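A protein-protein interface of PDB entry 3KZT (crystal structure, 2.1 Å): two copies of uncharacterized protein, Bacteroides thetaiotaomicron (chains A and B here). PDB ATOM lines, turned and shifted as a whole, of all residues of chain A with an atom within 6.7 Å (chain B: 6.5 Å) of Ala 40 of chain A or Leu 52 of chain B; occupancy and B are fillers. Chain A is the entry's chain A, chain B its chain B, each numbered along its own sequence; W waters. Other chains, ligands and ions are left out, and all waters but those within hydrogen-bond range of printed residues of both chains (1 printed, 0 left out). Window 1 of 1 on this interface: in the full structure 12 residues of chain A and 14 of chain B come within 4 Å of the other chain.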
ATOM      1  N   TYR A  35      10.505  -6.964 -29.084  1.00  0.00           N
ATOM      2  CA  TYR A  35      11.691  -6.121 -29.365  1.00  0.00           C
ATOM      3  C   TYR A  35      12.798  -6.211 -28.319  1.00  0.00           C
ATOM      4  O   TYR A  35      13.973  -6.217 -28.679  1.00  0.00           O
ATOM      5  CB  TYR A  35      11.303  -4.648 -29.659  1.00  0.00           C
ATOM      6  CG  TYR A  35      10.947  -4.443 -31.105  1.00  0.00           C
ATOM      7  CD1 TYR A  35       9.657  -4.699 -31.576  1.00  0.00           C
ATOM      8  CD2 TYR A  35      11.910  -4.026 -32.022  1.00  0.00           C
ATOM      9  CE1 TYR A  35       9.329  -4.539 -32.919  1.00  0.00           C
ATOM     10  CE2 TYR A  35      11.601  -3.858 -33.361  1.00  0.00           C
ATOM     11  CZ  TYR A  35      10.307  -4.111 -33.813  1.00  0.00           C
ATOM     12  OH  TYR A  35       9.984  -3.947 -35.134  1.00  0.00           O
ATOM     13  N   GLU A  36      12.430  -6.300 -27.041  1.00  0.00           N
ATOM     14  CA  GLU A  36      13.431  -6.488 -25.967  1.00  0.00           C
ATOM     15  C   GLU A  36      14.106  -7.868 -26.042  1.00  0.00           C
ATOM     16  O   GLU A  36      15.332  -7.961 -25.901  1.00  0.00           O
ATOM     17  CB  GLU A  36      12.826  -6.230 -24.592  1.00  0.00           C
ATOM     18  CG  GLU A  36      12.592  -4.744 -24.355  1.00  0.00           C
ATOM     19  CD  GLU A  36      11.684  -4.437 -23.188  1.00  0.00           C
ATOM     20  OE1 GLU A  36      11.452  -5.319 -22.312  1.00  0.00           O
ATOM     21  OE2 GLU A  36      11.194  -3.285 -23.143  1.00  0.00           O
ATOM     22  N   ALA A  37      13.306  -8.918 -26.287  1.00  0.00           N
ATOM     23  CA  ALA A  37      13.821 -10.298 -26.457  1.00  0.00           C
ATOM     24  C   ALA A  37      14.698 -10.418 -27.707  1.00  0.00           C
ATOM     25  O   ALA A  37      15.793 -10.968 -27.646  1.00  0.00           O
ATOM     26  CB  ALA A  37      12.666 -11.288 -26.538  1.00  0.00           C
ATOM     27  N   TYR A  38      14.194  -9.891 -28.826  1.00  0.00           N
ATOM     28  CA  TYR A  38      14.913  -9.895 -30.111  1.00  0.00           C
ATOM     29  C   TYR A  38      16.239  -9.112 -30.038  1.00  0.00           C
ATOM     30  O   TYR A  38      17.266  -9.598 -30.499  1.00  0.00           O
ATOM     31  CB  TYR A  38      14.020  -9.335 -31.228  1.00  0.00           C
ATOM     32  CG  TYR A  38      14.565  -9.537 -32.614  1.00  0.00           C
ATOM     33  CD1 TYR A  38      14.681 -10.823 -33.148  1.00  0.00           C
ATOM     34  CD2 TYR A  38      14.932  -8.446 -33.421  1.00  0.00           C
ATOM     35  CE1 TYR A  38      15.179 -11.032 -34.432  1.00  0.00           C
ATOM     36  CE2 TYR A  38      15.432  -8.643 -34.709  1.00  0.00           C
ATOM     37  CZ  TYR A  38      15.545  -9.941 -35.209  1.00  0.00           C
ATOM     38  OH  TYR A  38      16.026 -10.157 -36.464  1.00  0.00           O
ATOM     39  N   ALA A  39      16.197  -7.924 -29.431  1.00  0.00           N
ATOM     40  CA  ALA A  39      17.419  -7.073 -29.230  1.00  0.00           C
ATOM     41  C   ALA A  39      18.527  -7.763 -28.459  1.00  0.00           C
ATOM     42  O   ALA A  39      19.692  -7.578 -28.778  1.00  0.00           O
ATOM     43  CB  ALA A  39      17.073  -5.824 -28.536  1.00  0.00           C
ATOM     44  N   ALA A  40      18.157  -8.541 -27.433  1.00  0.00           N
ATOM     45  CA  ALA A  40      19.129  -9.314 -26.643  1.00  0.00           C
ATOM     46  C   ALA A  40      19.886 -10.375 -27.471  1.00  0.00           C
ATOM     47  O   ALA A  40      21.029 -10.683 -27.157  1.00  0.00           O
ATOM     48  CB  ALA A  40      18.443  -9.968 -25.429  1.00  0.00           C
ATOM     49  N   SER A  41      19.252 -10.911 -28.524  1.00  0.00           N
ATOM     50  CA  SER A  41      19.915 -11.878 -29.434  1.00  0.00           C
ATOM     51  C   SER A  41      21.131 -11.291 -30.186  1.00  0.00           C
ATOM     52  O   SER A  41      22.023 -12.034 -30.574  1.00  0.00           O
ATOM     53  CB  SER A  41      18.918 -12.482 -30.438  1.00  0.00           C
ATOM     54  OG  SER A  41      18.598 -11.572 -31.471  1.00  0.00           O
ATOM     55  N   PHE A  42      21.166  -9.964 -30.364  1.00  0.00           N
ATOM     56  CA  PHE A  42      22.334  -9.281 -30.938  1.00  0.00           C
ATOM     57  C   PHE A  42      23.564  -9.227 -29.996  1.00  0.00           C
ATOM     58  O   PHE A  42      24.647  -8.870 -30.463  1.00  0.00           O
ATOM     59  CB  PHE A  42      21.974  -7.863 -31.389  1.00  0.00           C
ATOM     60  CG  PHE A  42      21.049  -7.823 -32.553  1.00  0.00           C
ATOM     61  CD1 PHE A  42      19.670  -7.878 -32.369  1.00  0.00           C
ATOM     62  CD2 PHE A  42      21.554  -7.726 -33.857  1.00  0.00           C
ATOM     63  CE1 PHE A  42      18.811  -7.838 -33.447  1.00  0.00           C
ATOM     64  CE2 PHE A  42      20.700  -7.688 -34.945  1.00  0.00           C
ATOM     65  CZ  PHE A  42      19.326  -7.742 -34.744  1.00  0.00           C
ATOM     66  N   MET A  43      23.406  -9.564 -28.693  1.00  0.00           N
ATOM     67  CA  MET A  43      24.525  -9.566 -27.709  1.00  0.00           C
ATOM     68  C   MET A  43      25.515 -10.716 -27.976  1.00  0.00           C
ATOM     69  O   MET A  43      26.702 -10.596 -27.688  1.00  0.00           O
ATOM     70  CB  MET A  43      23.993  -9.700 -26.263  1.00  0.00           C
ATOM     71  CG  MET A  43      23.049  -8.576 -25.778  1.00  0.00           C
ATOM     72  SD  MET A  43      23.956  -6.897 -25.533  1.00  0.00           S
ATOM     73  CE  MET A  43      25.406  -7.481 -24.382  1.00  0.00           C
ATOM     74  N   SER A  44      25.004 -11.848 -28.487  1.00  0.00           N
ATOM     75  CA  SER A  44      25.852 -13.012 -28.849  1.00  0.00           C
ATOM     76  C   SER A  44      26.438 -12.782 -30.261  1.00  0.00           C
ATOM     77  O   SER A  44      25.763 -12.207 -31.122  1.00  0.00           O
ATOM     78  CB  SER A  44      25.027 -14.302 -28.836  1.00  0.00           C
ATOM     79  N   GLU A  48      24.289 -19.195 -32.221  1.00  0.00           N
ATOM     80  CA  GLU A  48      23.223 -18.979 -31.222  1.00  0.00           C
ATOM     81  C   GLU A  48      22.527 -17.599 -31.297  1.00  0.00           C
ATOM     82  O   GLU A  48      21.380 -17.475 -30.835  1.00  0.00           O
ATOM     83  CB  GLU A  48      23.794 -19.158 -29.810  1.00  0.00           C
ATOM     84  CG  GLU A  48      24.771 -18.037 -29.389  1.00  0.00           C
ATOM     85  CD  GLU A  48      25.783 -18.512 -28.410  1.00  0.00           C
ATOM     86  OE1 GLU A  48      26.761 -19.161 -28.835  1.00  0.00           O
ATOM     87  OE2 GLU A  48      25.609 -18.236 -27.212  1.00  0.00           O
ATOM     88  N   ALA A  49      23.235 -16.568 -31.825  1.00  0.00           N
ATOM     89  CA  ALA A  49      22.653 -15.225 -32.024  1.00  0.00           C
ATOM     90  C   ALA A  49      21.496 -15.322 -33.019  1.00  0.00           C
ATOM     91  O   ALA A  49      20.353 -14.951 -32.686  1.00  0.00           O
ATOM     92  CB  ALA A  49      23.714 -14.230 -32.525  1.00  0.00           C
ATOM     93  N   LEU A  52      18.630 -17.810 -31.738  1.00  0.00           N
ATOM     94  CA  LEU A  52      17.683 -17.172 -30.820  1.00  0.00           C
ATOM     95  C   LEU A  52      16.820 -16.146 -31.535  1.00  0.00           C
ATOM     96  O   LEU A  52      15.621 -16.073 -31.269  1.00  0.00           O
ATOM     97  CB  LEU A  52      18.383 -16.520 -29.619  1.00  0.00           C
ATOM     98  CG  LEU A  52      17.435 -16.103 -28.460  1.00  0.00           C
ATOM     99  CD1 LEU A  52      16.819 -17.299 -27.738  1.00  0.00           C
ATOM    100  CD2 LEU A  52      18.137 -15.231 -27.474  1.00  0.00           C
ATOM    101  N   ILE A  56      12.821 -16.413 -31.592  1.00  0.00           N
ATOM    102  CA  ILE A  56      11.974 -15.292 -31.169  1.00  0.00           C
ATOM    103  C   ILE A  56      11.006 -14.868 -32.293  1.00  0.00           C
ATOM    104  O   ILE A  56       9.822 -14.628 -32.028  1.00  0.00           O
ATOM    105  CB  ILE A  56      12.833 -14.092 -30.685  1.00  0.00           C
ATOM    106  CG1 ILE A  56      13.550 -14.451 -29.373  1.00  0.00           C
ATOM    107  CG2 ILE A  56      11.975 -12.859 -30.449  1.00  0.00           C
ATOM    108  CD1 ILE A  56      14.737 -13.580 -29.097  1.00  0.00           C
ATOM    109  N   LEU A  87      22.502  -3.522 -33.606  1.00  0.00           N
ATOM    110  CA  LEU A  87      22.042  -2.606 -32.579  1.00  0.00           C
ATOM    111  C   LEU A  87      23.202  -2.219 -31.695  1.00  0.00           C
ATOM    112  O   LEU A  87      24.005  -3.071 -31.320  1.00  0.00           O
ATOM    113  CB  LEU A  87      20.974  -3.282 -31.704  1.00  0.00           C
ATOM    114  CG  LEU A  87      19.639  -3.616 -32.357  1.00  0.00           C
ATOM    115  CD1 LEU A  87      18.830  -4.546 -31.480  1.00  0.00           C
ATOM    116  CD2 LEU A  87      18.863  -2.339 -32.659  1.00  0.00           C
ATOM    117  N   MET A  92      17.877   0.069 -27.580  1.00  0.00           N
ATOM    118  CA  MET A  92      16.579  -0.374 -27.007  1.00  0.00           C
ATOM    119  C   MET A  92      16.127   0.315 -25.748  1.00  0.00           C
ATOM    120  O   MET A  92      14.954   0.221 -25.422  1.00  0.00           O
ATOM    121  CB  MET A  92      16.508  -1.888 -26.829  1.00  0.00           C
ATOM    122  CG  MET A  92      16.319  -2.623 -28.086  1.00  0.00           C
ATOM    123  SD  MET A  92      14.767  -2.184 -29.151  1.00  0.00           S
ATOM    124  CE  MET A  92      15.579  -2.457 -30.926  1.00  0.00           C
ATOM    125  N   GLU B  36      20.098  -5.914 -17.526  1.00  0.00           N
ATOM    126  CA  GLU B  36      19.074  -5.692 -18.570  1.00  0.00           C
ATOM    127  C   GLU B  36      19.182  -6.724 -19.705  1.00  0.00           C
ATOM    128  O   GLU B  36      18.170  -7.245 -20.160  1.00  0.00           O
ATOM    129  CB  GLU B  36      19.153  -4.258 -19.116  1.00  0.00           C
ATOM    130  CG  GLU B  36      18.674  -3.218 -18.113  1.00  0.00           C
ATOM    131  CD  GLU B  36      18.989  -1.780 -18.515  1.00  0.00           C
ATOM    132  OE1 GLU B  36      19.315  -1.520 -19.696  1.00  0.00           O
ATOM    133  OE2 GLU B  36      18.903  -0.897 -17.630  1.00  0.00           O
ATOM    134  N   ALA B  37      20.413  -7.025 -20.135  1.00  0.00           N
ATOM    135  CA  ALA B  37      20.658  -8.040 -21.199  1.00  0.00           C
ATOM    136  C   ALA B  37      20.340  -9.452 -20.714  1.00  0.00           C
ATOM    137  O   ALA B  37      19.649 -10.211 -21.400  1.00  0.00           O
ATOM    138  CB  ALA B  37      22.076  -7.980 -21.646  1.00  0.00           C
ATOM    139  N   TYR B  38      20.873  -9.793 -19.540  1.00  0.00           N
ATOM    140  CA  TYR B  38      20.632 -11.103 -18.888  1.00  0.00           C
ATOM    141  C   TYR B  38      19.131 -11.348 -18.629  1.00  0.00           C
ATOM    142  O   TYR B  38      18.638 -12.425 -18.912  1.00  0.00           O
ATOM    143  CB  TYR B  38      21.455 -11.229 -17.579  1.00  0.00           C
ATOM    144  CG  TYR B  38      21.479 -12.630 -17.001  1.00  0.00           C
ATOM    145  CD1 TYR B  38      22.175 -13.658 -17.655  1.00  0.00           C
ATOM    146  CD2 TYR B  38      20.822 -12.933 -15.794  1.00  0.00           C
ATOM    147  CE1 TYR B  38      22.205 -14.948 -17.148  1.00  0.00           C
ATOM    148  CE2 TYR B  38      20.849 -14.240 -15.265  1.00  0.00           C
ATOM    149  CZ  TYR B  38      21.539 -15.243 -15.958  1.00  0.00           C
ATOM    150  OH  TYR B  38      21.583 -16.518 -15.464  1.00  0.00           O
ATOM    151  N   ALA B  40      16.646 -10.025 -20.318  1.00  0.00           N
ATOM    152  CA  ALA B  40      16.063 -10.217 -21.657  1.00  0.00           C
ATOM    153  C   ALA B  40      16.194 -11.654 -22.189  1.00  0.00           C
ATOM    154  O   ALA B  40      15.362 -12.082 -22.970  1.00  0.00           O
ATOM    155  CB  ALA B  40      16.658  -9.215 -22.657  1.00  0.00           C
ATOM    156  N   SER B  41      17.228 -12.392 -21.761  1.00  0.00           N
ATOM    157  CA  SER B  41      17.377 -13.817 -22.135  1.00  0.00           C
ATOM    158  C   SER B  41      16.242 -14.720 -21.578  1.00  0.00           C
ATOM    159  O   SER B  41      15.933 -15.744 -22.183  1.00  0.00           O
ATOM    160  CB  SER B  41      18.750 -14.362 -21.703  1.00  0.00           C
ATOM    161  OG  SER B  41      18.839 -14.506 -20.299  1.00  0.00           O
ATOM    162  N   SER B  44      12.770 -15.397 -23.745  1.00  0.00           N
ATOM    163  CA  SER B  44      12.759 -16.551 -24.659  1.00  0.00           C
ATOM    164  C   SER B  44      12.998 -17.834 -23.835  1.00  0.00           C
ATOM    165  O   SER B  44      13.501 -17.776 -22.707  1.00  0.00           O
ATOM    166  CB  SER B  44      13.824 -16.375 -25.755  1.00  0.00           C
ATOM    167  OG  SER B  44      15.031 -15.839 -25.222  1.00  0.00           O
ATOM    168  N   LYS B  47      17.109 -24.059 -25.154  1.00  0.00           N
ATOM    169  CA  LYS B  47      18.598 -24.041 -25.214  1.00  0.00           C
ATOM    170  C   LYS B  47      19.193 -22.726 -25.753  1.00  0.00           C
ATOM    171  O   LYS B  47      20.280 -22.311 -25.316  1.00  0.00           O
ATOM    172  CB  LYS B  47      19.155 -25.254 -26.020  1.00  0.00           C
ATOM    173  CG  LYS B  47      18.806 -25.304 -27.527  1.00  0.00           C
ATOM    174  CD  LYS B  47      19.641 -26.362 -28.262  1.00  0.00           C
ATOM    175  CE  LYS B  47      19.415 -26.287 -29.765  1.00  0.00           C
ATOM    176  NZ  LYS B  47      20.336 -27.156 -30.550  1.00  0.00           N
ATOM    177  N   GLU B  48      18.467 -22.080 -26.682  1.00  0.00           N
ATOM    178  CA  GLU B  48      18.884 -20.807 -27.291  1.00  0.00           C
ATOM    179  C   GLU B  48      18.861 -19.660 -26.257  1.00  0.00           C
ATOM    180  O   GLU B  48      19.715 -18.788 -26.273  1.00  0.00           O
ATOM    181  CB  GLU B  48      17.990 -20.449 -28.510  1.00  0.00           C
ATOM    182  CG  GLU B  48      18.138 -21.386 -29.785  1.00  0.00           C
ATOM    183  CD  GLU B  48      17.366 -22.737 -29.712  1.00  0.00           C
ATOM    184  OE1 GLU B  48      16.717 -23.030 -28.677  1.00  0.00           O
ATOM    185  OE2 GLU B  48      17.426 -23.503 -30.701  1.00  0.00           O
ATOM    186  N   ALA B  49      17.860 -19.673 -25.371  1.00  0.00           N
ATOM    187  CA  ALA B  49      17.764 -18.675 -24.268  1.00  0.00           C
ATOM    188  C   ALA B  49      18.926 -18.860 -23.273  1.00  0.00           C
ATOM    189  O   ALA B  49      19.578 -17.872 -22.901  1.00  0.00           O
ATOM    190  CB  ALA B  49      16.422 -18.795 -23.536  1.00  0.00           C
ATOM    191  N   LEU B  50      19.169 -20.121 -22.863  1.00  0.00           N
ATOM    192  CA  LEU B  50      20.275 -20.466 -21.943  1.00  0.00           C
ATOM    193  C   LEU B  50      21.645 -20.129 -22.554  1.00  0.00           C
ATOM    194  O   LEU B  50      22.533 -19.616 -21.858  1.00  0.00           O
ATOM    195  CB  LEU B  50      20.225 -21.960 -21.575  1.00  0.00           C
ATOM    196  CG  LEU B  50      21.224 -22.460 -20.521  1.00  0.00           C
ATOM    197  CD1 LEU B  50      21.170 -21.582 -19.274  1.00  0.00           C
ATOM    198  CD2 LEU B  50      20.946 -23.911 -20.179  1.00  0.00           C
ATOM    199  N   ALA B  51      21.807 -20.434 -23.857  1.00  0.00           N
ATOM    200  CA  ALA B  51      23.046 -20.124 -24.601  1.00  0.00           C
ATOM    201  C   ALA B  51      23.346 -18.608 -24.598  1.00  0.00           C
ATOM    202  O   ALA B  51      24.499 -18.222 -24.430  1.00  0.00           O
ATOM    203  CB  ALA B  51      22.975 -20.656 -26.041  1.00  0.00           C
ATOM    204  N   LEU B  52      22.296 -17.775 -24.756  1.00  0.00           N
ATOM    205  CA  LEU B  52      22.431 -16.314 -24.679  1.00  0.00           C
ATOM    206  C   LEU B  52      22.826 -15.883 -23.267  1.00  0.00           C
ATOM    207  O   LEU B  52      23.708 -15.041 -23.122  1.00  0.00           O
ATOM    208  CB  LEU B  52      21.136 -15.586 -25.111  1.00  0.00           C
ATOM    209  CG  LEU B  52      21.192 -14.027 -25.145  1.00  0.00           C
ATOM    210  CD1 LEU B  52      22.162 -13.532 -26.179  1.00  0.00           C
ATOM    211  CD2 LEU B  52      19.815 -13.431 -25.380  1.00  0.00           C
ATOM    212  N   GLY B  53      22.158 -16.450 -22.245  1.00  0.00           N
ATOM    213  CA  GLY B  53      22.501 -16.210 -20.835  1.00  0.00           C
ATOM    214  C   GLY B  53      23.977 -16.465 -20.556  1.00  0.00           C
ATOM    215  O   GLY B  53      24.647 -15.623 -19.959  1.00  0.00           O
ATOM    216  N   ASP B  54      24.480 -17.602 -21.048  1.00  0.00           N
ATOM    217  CA  ASP B  54      25.912 -17.956 -20.933  1.00  0.00           C
ATOM    218  C   ASP B  54      26.828 -17.002 -21.705  1.00  0.00           C
ATOM    219  O   ASP B  54      27.897 -16.656 -21.203  1.00  0.00           O
ATOM    220  CB  ASP B  54      26.170 -19.402 -21.403  1.00  0.00           C
ATOM    221  CG  ASP B  54      25.542 -20.467 -20.474  1.00  0.00           C
ATOM    222  OD1 ASP B  54      25.137 -20.151 -19.331  1.00  0.00           O
ATOM    223  OD2 ASP B  54      25.467 -21.632 -20.908  1.00  0.00           O
ATOM    224  N   SER B  55      26.412 -16.602 -22.921  1.00  0.00           N
ATOM    225  CA  SER B  55      27.152 -15.586 -23.722  1.00  0.00           C
ATOM    226  C   SER B  55      27.235 -14.251 -23.012  1.00  0.00           C
ATOM    227  O   SER B  55      28.303 -13.627 -23.005  1.00  0.00           O
ATOM    228  CB  SER B  55      26.534 -15.374 -25.112  1.00  0.00           C
ATOM    229  OG  SER B  55      26.911 -16.408 -25.979  1.00  0.00           O
ATOM    230  N   ILE B  56      26.107 -13.817 -22.438  1.00  0.00           N
ATOM    231  CA  ILE B  56      26.054 -12.565 -21.669  1.00  0.00           C
ATOM    232  C   ILE B  56      26.992 -12.664 -20.453  1.00  0.00           C
ATOM    233  O   ILE B  56      27.756 -11.747 -20.194  1.00  0.00           O
ATOM    234  CB  ILE B  56      24.595 -12.203 -21.234  1.00  0.00           C
ATOM    235  CG1 ILE B  56      23.744 -11.800 -22.451  1.00  0.00           C
ATOM    236  CG2 ILE B  56      24.596 -11.036 -20.252  1.00  0.00           C
ATOM    237  CD1 ILE B  56      24.087 -10.437 -23.019  1.00  0.00           C
ATOM    238  N   LYS B  57      26.934 -13.797 -19.727  1.00  0.00           N
ATOM    239  CA  LYS B  57      27.843 -14.048 -18.574  1.00  0.00           C
ATOM    240  C   LYS B  57      29.336 -13.960 -18.978  1.00  0.00           C
ATOM    241  O   LYS B  57      30.117 -13.329 -18.278  1.00  0.00           O
ATOM    242  CB  LYS B  57      27.579 -15.415 -17.936  1.00  0.00           C
ATOM    243  CG  LYS B  57      26.364 -15.489 -17.027  1.00  0.00           C
ATOM    244  CD  LYS B  57      26.153 -16.919 -16.625  1.00  0.00           C
ATOM    245  CE  LYS B  57      25.101 -17.093 -15.598  1.00  0.00           C
ATOM    246  NZ  LYS B  57      24.967 -18.549 -15.270  1.00  0.00           N
HETATM  247  O   HOH W   1      15.747 -13.147 -25.587  1.00  0.00           O
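OE2 of Glu 48 of chain A lies within hydrogen-bond range of OG of Ser 55 of chain B, at 2.6 Å.
The side-chain carboxylate of Glu 48 of chain A sits close to the backbone carbonyl oxygen of Ala 51 of chain B.
The side-chain hydroxyl (OG) of Ser 44 of chain B is in hydrogen-bond range of the backbone carbonyl oxygen (O) of Ser 41 of chain B (3.2 Å).
O of Ala 51 of chain B is in hydrogen-bond range of OG of Ser 55 of chain B (3.4 Å).
CB of Ala 40 of chain B touches O of Glu 36 of chain A (3.7 Å).
Ala 40 of chain A touches Ala 40 of chain B (CB to CB, 3.4 Å).
Leu 52 of chain B touches Ala 40 of chain A (CD1 to O, 3.2 Å).
Met 43 of chain A touches Ile 56 of chain B.
Ser 44 of chain A touches Leu 52 of chain B (CB to CD1, 3.98 Å).
CD1 of Leu 52 of chain A touches OG of Ser 44 of chain B (3.4 Å).
Leu 52 of chain A touches Glu 48 of chain B (CD1 to CB, 3.4 Å).
Leu 52 of chain A touches Ala 49 of chain B (CD1 to N, 3.5 Å).
Leu 52 of chain A touches Leu 52 of chain B (CD2 to CD2, 3.2 Å).
Ala 40 of chain A touches just these residues of chain B: Ala 40 (3.4 Å) and Leu 52 (3.2 Å).
Of the printed residues of chain A, Leu 52 of chain B touches Ala 40, Ser 44 and Leu 52.
Printed residues of chain A within 4 Å of Glu 48 of chain B: Leu 52.
Of the printed residues of chain A, Ala 51 of chain B touches Glu 48.
Of the printed residues of chain B, Glu 48 of chain A touches Ala 51 and Ser 55.
Ala 37 of chain A touches none of the printed residues of chain B.
The nearest residue of chain B that does not touch Ala 40 of chain A is Ala 37 of chain B (4.2 Å).
The nearest printed residue of chain A that does not touch Leu 52 of chain B is Ser 41 of chain A (4.1 Å).
Printed residues of chain A that touch a printed residue of chain B: Glu 36, Ala 40, Met 43, Ser 44, Glu 48 and Leu 52.
Printed residues of chain B that touch a printed residue of chain A: Ala 40, Ser 44, Glu 48, Ala 49, Ala 51, Leu 52, Ser 55 and Ile 56.
Hydrophobic or aromatic side chains of chain B that line the printed part of chain A: Ala 40, Ala 51, Leu 52 and Ile 56.
Ser 44 of chain A touches Leu 52 of chain B, and with the chains exchanged Leu 52 of chain A touches Ser 44 of chain B.
Leu 52 of chain A touches Glu 48 of chain B, but with the chains exchanged Glu 48 of chain A does not touch Leu 52 of chain B (4.1 Å).
Leu 52 of chain A touches Ala 49 of chain B, but with the chains exchanged Ala 49 of chain A does not touch Leu 52 of chain B (6.1 Å).
Leu 52 of chain B touches its own counterpart, Leu 52 of chain A.
Positions printed for both chains: 36, 37, 38, 40, 41, 44, 48, 49, 52 and 56.
Water W1 lies within hydrogen-bond range of OG of Ser 44 of chain B (2.8 Å), O of Ala 40 of chain B (2.9 Å) and O of Ala 37 of chain A (3.0 Å).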
